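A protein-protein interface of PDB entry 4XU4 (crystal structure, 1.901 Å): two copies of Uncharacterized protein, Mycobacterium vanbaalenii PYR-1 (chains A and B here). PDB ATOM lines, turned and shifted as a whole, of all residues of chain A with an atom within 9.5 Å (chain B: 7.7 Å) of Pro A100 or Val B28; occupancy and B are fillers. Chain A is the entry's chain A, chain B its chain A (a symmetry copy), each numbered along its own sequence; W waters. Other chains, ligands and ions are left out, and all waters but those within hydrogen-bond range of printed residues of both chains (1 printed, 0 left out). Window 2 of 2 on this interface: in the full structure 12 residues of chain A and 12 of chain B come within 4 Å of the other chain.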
ATOM      1  N   VAL A  96      -1.137  -0.482 -19.516  1.00  0.00           N
ATOM      2  CA  VAL A  96      -2.416  -0.591 -20.224  1.00  0.00           C
ATOM      3  C   VAL A  96      -3.050   0.738 -20.626  1.00  0.00           C
ATOM      4  O   VAL A  96      -4.170   0.754 -21.136  1.00  0.00           O
ATOM      5  CB  VAL A  96      -3.452  -1.414 -19.418  1.00  0.00           C
ATOM      6  CG1 VAL A  96      -2.903  -2.812 -19.109  1.00  0.00           C
ATOM      7  CG2 VAL A  96      -3.833  -0.683 -18.120  1.00  0.00           C
ATOM      8  N   HIS A  97      -2.334   1.842 -20.426  1.00  0.00           N
ATOM      9  CA  HIS A  97      -2.925   3.177 -20.594  1.00  0.00           C
ATOM     10  C   HIS A  97      -3.499   3.474 -21.985  1.00  0.00           C
ATOM     11  O   HIS A  97      -4.377   4.328 -22.121  1.00  0.00           O
ATOM     12  CB  HIS A  97      -1.904   4.263 -20.256  1.00  0.00           C
ATOM     13  CG  HIS A  97      -0.898   4.487 -21.342  1.00  0.00           C
ATOM     14  ND1 HIS A  97       0.242   3.726 -21.468  1.00  0.00           N
ATOM     15  CD2 HIS A  97      -0.875   5.376 -22.364  1.00  0.00           C
ATOM     16  CE1 HIS A  97       0.933   4.143 -22.515  1.00  0.00           C
ATOM     17  NE2 HIS A  97       0.275   5.142 -23.076  1.00  0.00           N
ATOM     18  N   ALA A  98      -3.006   2.791 -23.013  1.00  0.00           N
ATOM     19  CA  ALA A  98      -3.461   3.049 -24.387  1.00  0.00           C
ATOM     20  C   ALA A  98      -4.760   2.324 -24.748  1.00  0.00           C
ATOM     21  O   ALA A  98      -5.314   2.545 -25.820  1.00  0.00           O
ATOM     22  CB  ALA A  98      -2.367   2.696 -25.389  1.00  0.00           C
ATOM     23  N   PHE A  99      -5.238   1.455 -23.861  1.00  0.00           N
ATOM     24  CA  PHE A  99      -6.456   0.677 -24.115  1.00  0.00           C
ATOM     25  C   PHE A  99      -7.694   1.518 -23.806  1.00  0.00           C
ATOM     26  O   PHE A  99      -7.573   2.579 -23.184  1.00  0.00           O
ATOM     27  CB  PHE A  99      -6.434  -0.608 -23.274  1.00  0.00           C
ATOM     28  CG  PHE A  99      -5.515  -1.673 -23.813  1.00  0.00           C
ATOM     29  CD1 PHE A  99      -5.977  -2.600 -24.732  1.00  0.00           C
ATOM     30  CD2 PHE A  99      -4.200  -1.754 -23.386  1.00  0.00           C
ATOM     31  CE1 PHE A  99      -5.140  -3.587 -25.228  1.00  0.00           C
ATOM     32  CE2 PHE A  99      -3.354  -2.737 -23.875  1.00  0.00           C
ATOM     33  CZ  PHE A  99      -3.828  -3.657 -24.798  1.00  0.00           C
ATOM     34  N   PRO A 100      -8.892   1.060 -24.230  1.00  0.00           N
ATOM     35  CA  PRO A 100     -10.106   1.865 -24.016  1.00  0.00           C
ATOM     36  C   PRO A 100     -10.373   2.170 -22.543  1.00  0.00           C
ATOM     37  O   PRO A 100     -10.100   1.333 -21.679  1.00  0.00           O
ATOM     38  CB  PRO A 100     -11.212   0.982 -24.596  1.00  0.00           C
ATOM     39  CG  PRO A 100     -10.519   0.218 -25.689  1.00  0.00           C
ATOM     40  CD  PRO A 100      -9.155  -0.092 -25.116  1.00  0.00           C
ATOM     41  N   VAL A 101     -10.920   3.352 -22.273  1.00  0.00           N
ATOM     42  CA  VAL A 101     -11.025   3.883 -20.916  1.00  0.00           C
ATOM     43  C   VAL A 101     -11.828   3.014 -19.929  1.00  0.00           C
ATOM     44  O   VAL A 101     -11.464   2.912 -18.757  1.00  0.00           O
ATOM     45  CB  VAL A 101     -11.576   5.332 -20.939  1.00  0.00           C
ATOM     46  CG1 VAL A 101     -12.993   5.364 -21.514  1.00  0.00           C
ATOM     47  CG2 VAL A 101     -11.548   5.949 -19.558  1.00  0.00           C
ATOM     48  N   VAL A 102     -12.905   2.384 -20.389  1.00  0.00           N
ATOM     49  CA  VAL A 102     -13.739   1.601 -19.477  1.00  0.00           C
ATOM     50  C   VAL A 102     -13.034   0.353 -18.931  1.00  0.00           C
ATOM     51  O   VAL A 102     -12.949   0.200 -17.721  1.00  0.00           O
ATOM     52  CB  VAL A 102     -15.126   1.245 -20.074  1.00  0.00           C
ATOM     53  CG1 VAL A 102     -15.834   0.206 -19.188  1.00  0.00           C
ATOM     54  CG2 VAL A 102     -15.975   2.496 -20.204  1.00  0.00           C
ATOM     55  N   PRO A 103     -12.530  -0.535 -19.806  1.00  0.00           N
ATOM     56  CA  PRO A 103     -11.853  -1.681 -19.192  1.00  0.00           C
ATOM     57  C   PRO A 103     -10.630  -1.286 -18.357  1.00  0.00           C
ATOM     58  O   PRO A 103     -10.419  -1.883 -17.302  1.00  0.00           O
ATOM     59  CB  PRO A 103     -11.446  -2.552 -20.390  1.00  0.00           C
ATOM     60  CG  PRO A 103     -11.517  -1.635 -21.588  1.00  0.00           C
ATOM     61  CD  PRO A 103     -12.592  -0.647 -21.279  1.00  0.00           C
ATOM     62  N   VAL A 104      -9.855  -0.300 -18.805  1.00  0.00           N
ATOM     63  CA  VAL A 104      -8.695   0.150 -18.027  1.00  0.00           C
ATOM     64  C   VAL A 104      -9.102   0.665 -16.653  1.00  0.00           C
ATOM     65  O   VAL A 104      -8.539   0.268 -15.632  1.00  0.00           O
ATOM     66  CB  VAL A 104      -7.901   1.255 -18.760  1.00  0.00           C
ATOM     67  CG1 VAL A 104      -6.891   1.894 -17.815  1.00  0.00           C
ATOM     68  CG2 VAL A 104      -7.202   0.665 -19.985  1.00  0.00           C
ATOM     69  N   THR A 105     -10.084   1.556 -16.620  1.00  0.00           N
ATOM     70  CA  THR A 105     -10.526   2.111 -15.350  1.00  0.00           C
ATOM     71  C   THR A 105     -11.176   1.038 -14.461  1.00  0.00           C
ATOM     72  O   THR A 105     -10.957   1.021 -13.251  1.00  0.00           O
ATOM     73  CB  THR A 105     -11.493   3.278 -15.566  1.00  0.00           C
ATOM     74  OG1 THR A 105     -10.936   4.172 -16.539  1.00  0.00           O
ATOM     75  CG2 THR A 105     -11.729   4.017 -14.262  1.00  0.00           C
ATOM     76  N   ALA A 106     -11.954   0.140 -15.061  1.00  0.00           N
ATOM     77  CA  ALA A 106     -12.574  -0.951 -14.287  1.00  0.00           C
ATOM     78  C   ALA A 106     -11.526  -1.861 -13.645  1.00  0.00           C
ATOM     79  O   ALA A 106     -11.703  -2.323 -12.511  1.00  0.00           O
ATOM     80  CB  ALA A 106     -13.518  -1.767 -15.165  1.00  0.00           C
ATOM     81  N   LEU A 107     -10.434  -2.117 -14.362  1.00  0.00           N
ATOM     82  CA  LEU A 107      -9.382  -2.992 -13.846  1.00  0.00           C
ATOM     83  C   LEU A 107      -8.732  -2.369 -12.615  1.00  0.00           C
ATOM     84  O   LEU A 107      -8.508  -3.040 -11.612  1.00  0.00           O
ATOM     85  CB  LEU A 107      -8.326  -3.267 -14.926  1.00  0.00           C
ATOM     86  CG  LEU A 107      -7.085  -4.045 -14.472  1.00  0.00           C
ATOM     87  CD1 LEU A 107      -7.481  -5.433 -13.985  1.00  0.00           C
ATOM     88  CD2 LEU A 107      -6.056  -4.156 -15.613  1.00  0.00           C
ATOM     89  N   VAL A 108      -8.456  -1.071 -12.685  1.00  0.00           N
ATOM     90  CA  VAL A 108      -7.856  -0.369 -11.558  1.00  0.00           C
ATOM     91  C   VAL A 108      -8.825  -0.273 -10.371  1.00  0.00           C
ATOM     92  O   VAL A 108      -8.418  -0.421  -9.221  1.00  0.00           O
ATOM     93  CB  VAL A 108      -7.344   1.030 -11.977  1.00  0.00           C
ATOM     94  CG1 VAL A 108      -6.626   1.714 -10.799  1.00  0.00           C
ATOM     95  CG2 VAL A 108      -6.384   0.885 -13.150  1.00  0.00           C
ATOM     96  N   ASP A 153      -5.116   9.355 -25.115  1.00  0.00           N
ATOM     97  CA  ASP A 153      -6.020   8.245 -24.826  1.00  0.00           C
ATOM     98  C   ASP A 153      -6.161   7.958 -23.326  1.00  0.00           C
ATOM     99  O   ASP A 153      -6.776   6.972 -22.936  1.00  0.00           O
ATOM    100  CB  ASP A 153      -5.606   6.988 -25.597  1.00  0.00           C
ATOM    101  CG  ASP A 153      -5.903   7.094 -27.090  1.00  0.00           C
ATOM    102  OD1 ASP A 153      -6.905   7.753 -27.453  1.00  0.00           O
ATOM    103  OD2 ASP A 153      -5.137   6.524 -27.899  1.00  0.00           O
ATOM    104  N   SER A 154      -5.611   8.838 -22.493  1.00  0.00           N
ATOM    105  CA  SER A 154      -5.672   8.666 -21.041  1.00  0.00           C
ATOM    106  C   SER A 154      -5.914   9.988 -20.330  1.00  0.00           C
ATOM    107  O   SER A 154      -5.339  10.229 -19.270  1.00  0.00           O
ATOM    108  CB  SER A 154      -4.365   8.064 -20.514  1.00  0.00           C
ATOM    109  OG  SER A 154      -3.894   7.045 -21.374  1.00  0.00           O
ATOM    110  N   PRO A 162      -8.817   8.867 -15.813  1.00  0.00           N
ATOM    111  CA  PRO A 162      -9.851   8.425 -14.864  1.00  0.00           C
ATOM    112  C   PRO A 162      -9.324   7.387 -13.863  1.00  0.00           C
ATOM    113  O   PRO A 162      -9.813   7.332 -12.734  1.00  0.00           O
ATOM    114  CB  PRO A 162     -10.926   7.818 -15.776  1.00  0.00           C
ATOM    115  CG  PRO A 162     -10.766   8.588 -17.089  1.00  0.00           C
ATOM    116  CD  PRO A 162      -9.272   8.813 -17.217  1.00  0.00           C
ATOM    117  N   PHE A 163      -8.328   6.589 -14.253  1.00  0.00           N
ATOM    118  CA  PHE A 163      -7.800   5.569 -13.336  1.00  0.00           C
ATOM    119  C   PHE A 163      -7.119   6.157 -12.098  1.00  0.00           C
ATOM    120  O   PHE A 163      -6.848   5.438 -11.146  1.00  0.00           O
ATOM    121  CB  PHE A 163      -6.890   4.532 -14.040  1.00  0.00           C
ATOM    122  CG  PHE A 163      -5.609   5.103 -14.629  1.00  0.00           C
ATOM    123  CD1 PHE A 163      -4.602   5.615 -13.809  1.00  0.00           C
ATOM    124  CD2 PHE A 163      -5.394   5.067 -15.999  1.00  0.00           C
ATOM    125  CE1 PHE A 163      -3.419   6.120 -14.356  1.00  0.00           C
ATOM    126  CE2 PHE A 163      -4.216   5.563 -16.555  1.00  0.00           C
ATOM    127  CZ  PHE A 163      -3.232   6.092 -15.731  1.00  0.00           C
ATOM    128  N   ILE B  21     -20.626  -3.909 -18.129  1.00  0.00           N
ATOM    129  CA  ILE B  21     -19.271  -3.352 -18.119  1.00  0.00           C
ATOM    130  C   ILE B  21     -18.318  -4.270 -18.884  1.00  0.00           C
ATOM    131  O   ILE B  21     -17.531  -3.822 -19.731  1.00  0.00           O
ATOM    132  CB  ILE B  21     -18.761  -3.151 -16.685  1.00  0.00           C
ATOM    133  CG1 ILE B  21     -19.572  -2.047 -15.996  1.00  0.00           C
ATOM    134  CG2 ILE B  21     -17.257  -2.824 -16.689  1.00  0.00           C
ATOM    135  CD1 ILE B  21     -19.378  -1.983 -14.479  1.00  0.00           C
ATOM    136  N   GLY B  22     -18.392  -5.561 -18.578  1.00  0.00           N
ATOM    137  CA  GLY B  22     -17.545  -6.547 -19.216  1.00  0.00           C
ATOM    138  C   GLY B  22     -17.849  -6.692 -20.695  1.00  0.00           C
ATOM    139  O   GLY B  22     -16.948  -6.795 -21.518  1.00  0.00           O
ATOM    140  N   ASP B  23     -19.125  -6.695 -21.049  1.00  0.00           N
ATOM    141  CA  ASP B  23     -19.477  -6.859 -22.454  1.00  0.00           C
ATOM    142  C   ASP B  23     -19.115  -5.618 -23.270  1.00  0.00           C
ATOM    143  O   ASP B  23     -18.666  -5.735 -24.403  1.00  0.00           O
ATOM    144  CB  ASP B  23     -20.954  -7.187 -22.603  1.00  0.00           C
ATOM    145  CG  ASP B  23     -21.275  -7.841 -23.936  1.00  0.00           C
ATOM    146  OD1 ASP B  23     -20.507  -8.723 -24.393  1.00  0.00           O
ATOM    147  OD2 ASP B  23     -22.310  -7.467 -24.529  1.00  0.00           O
ATOM    148  N   HIS B  24     -19.294  -4.433 -22.695  1.00  0.00           N
ATOM    149  CA  HIS B  24     -18.811  -3.231 -23.369  1.00  0.00           C
ATOM    150  C   HIS B  24     -17.298  -3.309 -23.605  1.00  0.00           C
ATOM    151  O   HIS B  24     -16.804  -2.917 -24.658  1.00  0.00           O
ATOM    152  CB  HIS B  24     -19.121  -1.966 -22.573  1.00  0.00           C
ATOM    153  CG  HIS B  24     -18.370  -0.776 -23.072  1.00  0.00           C
ATOM    154  ND1 HIS B  24     -18.736  -0.089 -24.206  1.00  0.00           N
ATOM    155  CD2 HIS B  24     -17.231  -0.187 -22.628  1.00  0.00           C
ATOM    156  CE1 HIS B  24     -17.879   0.894 -24.426  1.00  0.00           C
ATOM    157  NE2 HIS B  24     -16.947   0.847 -23.485  1.00  0.00           N
ATOM    158  N   SER B  25     -16.565  -3.830 -22.621  1.00  0.00           N
ATOM    159  CA  SER B  25     -15.122  -3.982 -22.764  1.00  0.00           C
ATOM    160  C   SER B  25     -14.768  -4.922 -23.915  1.00  0.00           C
ATOM    161  O   SER B  25     -13.870  -4.629 -24.705  1.00  0.00           O
ATOM    162  CB  SER B  25     -14.490  -4.465 -21.448  1.00  0.00           C
ATOM    163  OG  SER B  25     -14.694  -3.508 -20.421  1.00  0.00           O
ATOM    164  N   HIS B  26     -15.471  -6.044 -24.018  1.00  0.00           N
ATOM    165  CA  HIS B  26     -15.246  -6.971 -25.132  1.00  0.00           C
ATOM    166  C   HIS B  26     -15.573  -6.326 -26.483  1.00  0.00           C
ATOM    167  O   HIS B  26     -14.861  -6.538 -27.466  1.00  0.00           O
ATOM    168  CB  HIS B  26     -16.081  -8.249 -24.957  1.00  0.00           C
ATOM    169  CG  HIS B  26     -15.428  -9.274 -24.065  1.00  0.00           C
ATOM    170  ND1 HIS B  26     -16.052 -10.441 -23.713  1.00  0.00           N
ATOM    171  CD2 HIS B  26     -14.209  -9.289 -23.484  1.00  0.00           C
ATOM    172  CE1 HIS B  26     -15.235 -11.153 -22.932  1.00  0.00           C
ATOM    173  NE2 HIS B  26     -14.117 -10.469 -22.784  1.00  0.00           N
ATOM    174  N   VAL B  27     -16.647  -5.547 -26.539  1.00  0.00           N
ATOM    175  CA  VAL B  27     -17.038  -4.936 -27.816  1.00  0.00           C
ATOM    176  C   VAL B  27     -16.052  -3.851 -28.239  1.00  0.00           C
ATOM    177  O   VAL B  27     -15.577  -3.844 -29.382  1.00  0.00           O
ATOM    178  CB  VAL B  27     -18.467  -4.381 -27.756  1.00  0.00           C
ATOM    179  CG1 VAL B  27     -18.761  -3.488 -28.971  1.00  0.00           C
ATOM    180  CG2 VAL B  27     -19.470  -5.535 -27.678  1.00  0.00           C
ATOM    181  N   VAL B  28     -15.712  -2.964 -27.308  1.00  0.00           N
ATOM    182  CA  VAL B  28     -14.849  -1.828 -27.623  1.00  0.00           C
ATOM    183  C   VAL B  28     -13.417  -2.253 -27.957  1.00  0.00           C
ATOM    184  O   VAL B  28     -12.719  -1.556 -28.686  1.00  0.00           O
ATOM    185  CB  VAL B  28     -14.882  -0.742 -26.506  1.00  0.00           C
ATOM    186  CG1 VAL B  28     -14.075  -1.185 -25.266  1.00  0.00           C
ATOM    187  CG2 VAL B  28     -14.373   0.588 -27.036  1.00  0.00           C
ATOM    188  N   THR B  29     -12.987  -3.414 -27.465  1.00  0.00           N
ATOM    189  CA  THR B  29     -11.651  -3.908 -27.797  1.00  0.00           C
ATOM    190  C   THR B  29     -11.656  -4.826 -29.009  1.00  0.00           C
ATOM    191  O   THR B  29     -10.601  -5.265 -29.459  1.00  0.00           O
ATOM    192  CB  THR B  29     -11.024  -4.707 -26.641  1.00  0.00           C
ATOM    193  OG1 THR B  29     -11.910  -5.779 -26.286  1.00  0.00           O
ATOM    194  CG2 THR B  29     -10.784  -3.811 -25.440  1.00  0.00           C
ATOM    195  N   GLY B  30     -12.837  -5.149 -29.517  1.00  0.00           N
ATOM    196  CA  GLY B  30     -12.923  -6.041 -30.662  1.00  0.00           C
ATOM    197  C   GLY B  30     -12.822  -7.514 -30.292  1.00  0.00           C
ATOM    198  O   GLY B  30     -12.601  -8.366 -31.157  1.00  0.00           O
ATOM    199  N   THR B  31     -12.973  -7.821 -29.005  1.00  0.00           N
ATOM    200  CA  THR B  31     -12.994  -9.220 -28.582  1.00  0.00           C
ATOM    201  C   THR B  31     -14.213  -9.917 -29.186  1.00  0.00           C
ATOM    202  O   THR B  31     -14.130 -11.057 -29.632  1.00  0.00           O
ATOM    203  CB  THR B  31     -13.037  -9.358 -27.044  1.00  0.00           C
ATOM    204  OG1 THR B  31     -11.934  -8.647 -26.469  1.00  0.00           O
ATOM    205  CG2 THR B  31     -12.962 -10.836 -26.634  1.00  0.00           C
ATOM    206  N   THR B  32     -15.346  -9.216 -29.188  1.00  0.00           N
ATOM    207  CA  THR B  32     -16.575  -9.733 -29.793  1.00  0.00           C
ATOM    208  C   THR B  32     -17.214  -8.653 -30.665  1.00  0.00           C
ATOM    209  O   THR B  32     -16.901  -7.470 -30.523  1.00  0.00           O
ATOM    210  CB  THR B  32     -17.614 -10.149 -28.735  1.00  0.00           C
ATOM    211  OG1 THR B  32     -17.918  -9.023 -27.902  1.00  0.00           O
ATOM    212  CG2 THR B  32     -17.092 -11.293 -27.868  1.00  0.00           C
ATOM    213  N   SER B  44     -23.551  -1.183 -24.952  1.00  0.00           N
ATOM    214  CA  SER B  44     -23.015  -1.909 -26.104  1.00  0.00           C
ATOM    215  C   SER B  44     -23.642  -3.291 -26.326  1.00  0.00           C
ATOM    216  O   SER B  44     -23.224  -4.030 -27.217  1.00  0.00           O
ATOM    217  CB  SER B  44     -21.495  -2.054 -25.984  1.00  0.00           C
ATOM    218  OG  SER B  44     -20.874  -0.783 -25.892  1.00  0.00           O
ATOM    219  N   ALA B  94     -10.618  -8.807 -22.072  1.00  0.00           N
ATOM    220  CA  ALA B  94     -10.763  -7.851 -23.177  1.00  0.00           C
ATOM    221  C   ALA B  94      -9.410  -7.256 -23.560  1.00  0.00           C
ATOM    222  O   ALA B  94      -9.109  -7.038 -24.742  1.00  0.00           O
ATOM    223  CB  ALA B  94     -11.735  -6.750 -22.796  1.00  0.00           C
ATOM    224  N   LEU B  95      -8.585  -6.994 -22.554  1.00  0.00           N
ATOM    225  CA  LEU B  95      -7.276  -6.396 -22.790  1.00  0.00           C
ATOM    226  C   LEU B  95      -6.308  -7.360 -23.471  1.00  0.00           C
ATOM    227  O   LEU B  95      -5.507  -6.942 -24.295  1.00  0.00           O
ATOM    228  CB  LEU B  95      -6.668  -5.894 -21.471  1.00  0.00           C
ATOM    229  CG  LEU B  95      -7.463  -4.825 -20.725  1.00  0.00           C
ATOM    230  CD1 LEU B  95      -6.729  -4.374 -19.458  1.00  0.00           C
ATOM    231  CD2 LEU B  95      -7.734  -3.635 -21.633  1.00  0.00           C
ATOM    232  N   HIS B  97      -7.058 -10.368 -25.206  1.00  0.00           N
ATOM    233  CA  HIS B  97      -7.678 -11.354 -26.101  1.00  0.00           C
ATOM    234  C   HIS B  97      -6.907 -11.645 -27.396  1.00  0.00           C
ATOM    235  O   HIS B  97      -7.067 -12.717 -27.981  1.00  0.00           O
ATOM    236  CB  HIS B  97      -9.096 -10.925 -26.474  1.00  0.00           C
ATOM    237  CG  HIS B  97      -9.134  -9.846 -27.511  1.00  0.00           C
ATOM    238  ND1 HIS B  97      -9.020  -8.511 -27.198  1.00  0.00           N
ATOM    239  CD2 HIS B  97      -9.253  -9.911 -28.859  1.00  0.00           C
ATOM    240  CE1 HIS B  97      -9.079  -7.794 -28.308  1.00  0.00           C
ATOM    241  NE2 HIS B  97      -9.218  -8.621 -29.329  1.00  0.00           N
HETATM  242  O   HOH W   1     -14.312   2.362 -23.365  1.00  0.00           O
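Among the printed residues, merely in contact across the chains: Pro A103 with Ser B25, Phe A99 with Leu B95, Val A102 with His B24, Pro A100 with Val B28 and Leu A107 with Leu B95.
The side-chain hydroxyl of Ser B25 sits at hydrogen-bond distance from the backbone carbonyl oxygen of Ile B21, 2.9 Å away. OG of Ser B44 lies within hydrogen-bond range of ND1 of His B24 (2.8 Å). O of Ser B25 is in hydrogen-bond range of OG1 of Thr B29, at 2.8 Å.
Water W1 lies within hydrogen-bond range of NE2 of His B24 and N of Val A102.
Of the 16 printed residues of chain B, 4 touch a printed residue of chain A. Hydrophobic or aromatic side chains of chain B within 4 Å of the printed part of chain A: His B24, Val B28 and Leu B95. Of the 17 printed residues of chain A, 5 touch a printed residue of chain B. Hydrophobic or aromatic side chains of chain A within 4 Å of the printed part of chain B: Phe A99, Pro A100, Val A102, Pro A103 and Leu A107. Among the printed residues, 5 pairs touch across the chains. Among the printed residues, no Asp or Glu carboxylate lies within 4 Å of a Lys or Arg side-chain nitrogen of the other chain.
Position printed for both chains: 97. Of the 5 pairs that touch across the chains among the printed residues, none has its exchanged pair printed and touching as well.
Of the printed residues of chain B, Phe A99 touches Leu B95. Of chain B, only Val B28 comes within 4 Å of Pro A100. Printed residues of chain B within 4 Å of Val A102: His B24. Printed residues of chain B within 4 Å of Pro A103: Ser B25 (3.4 Å). Of the printed residues of chain A, His B24 touches Val A102 (3.6 Å). Ser B25 touches just one residue of chain A: Pro A103 (3.4 Å). No residue of chain A comes within 4 Å of Val B27. Of chain A, only Pro A100 (3.7 Å) comes within 4 Å of Val B28. No residue of chain A comes within 4 Å of Thr B29. Of the printed residues of chain A, Leu B95 touches Phe A99 (3.5 Å) and Leu A107 (3.9 Å). The nearest printed residue of chain B that does not touch Leu A107 is Ile B21 (7.2 Å).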
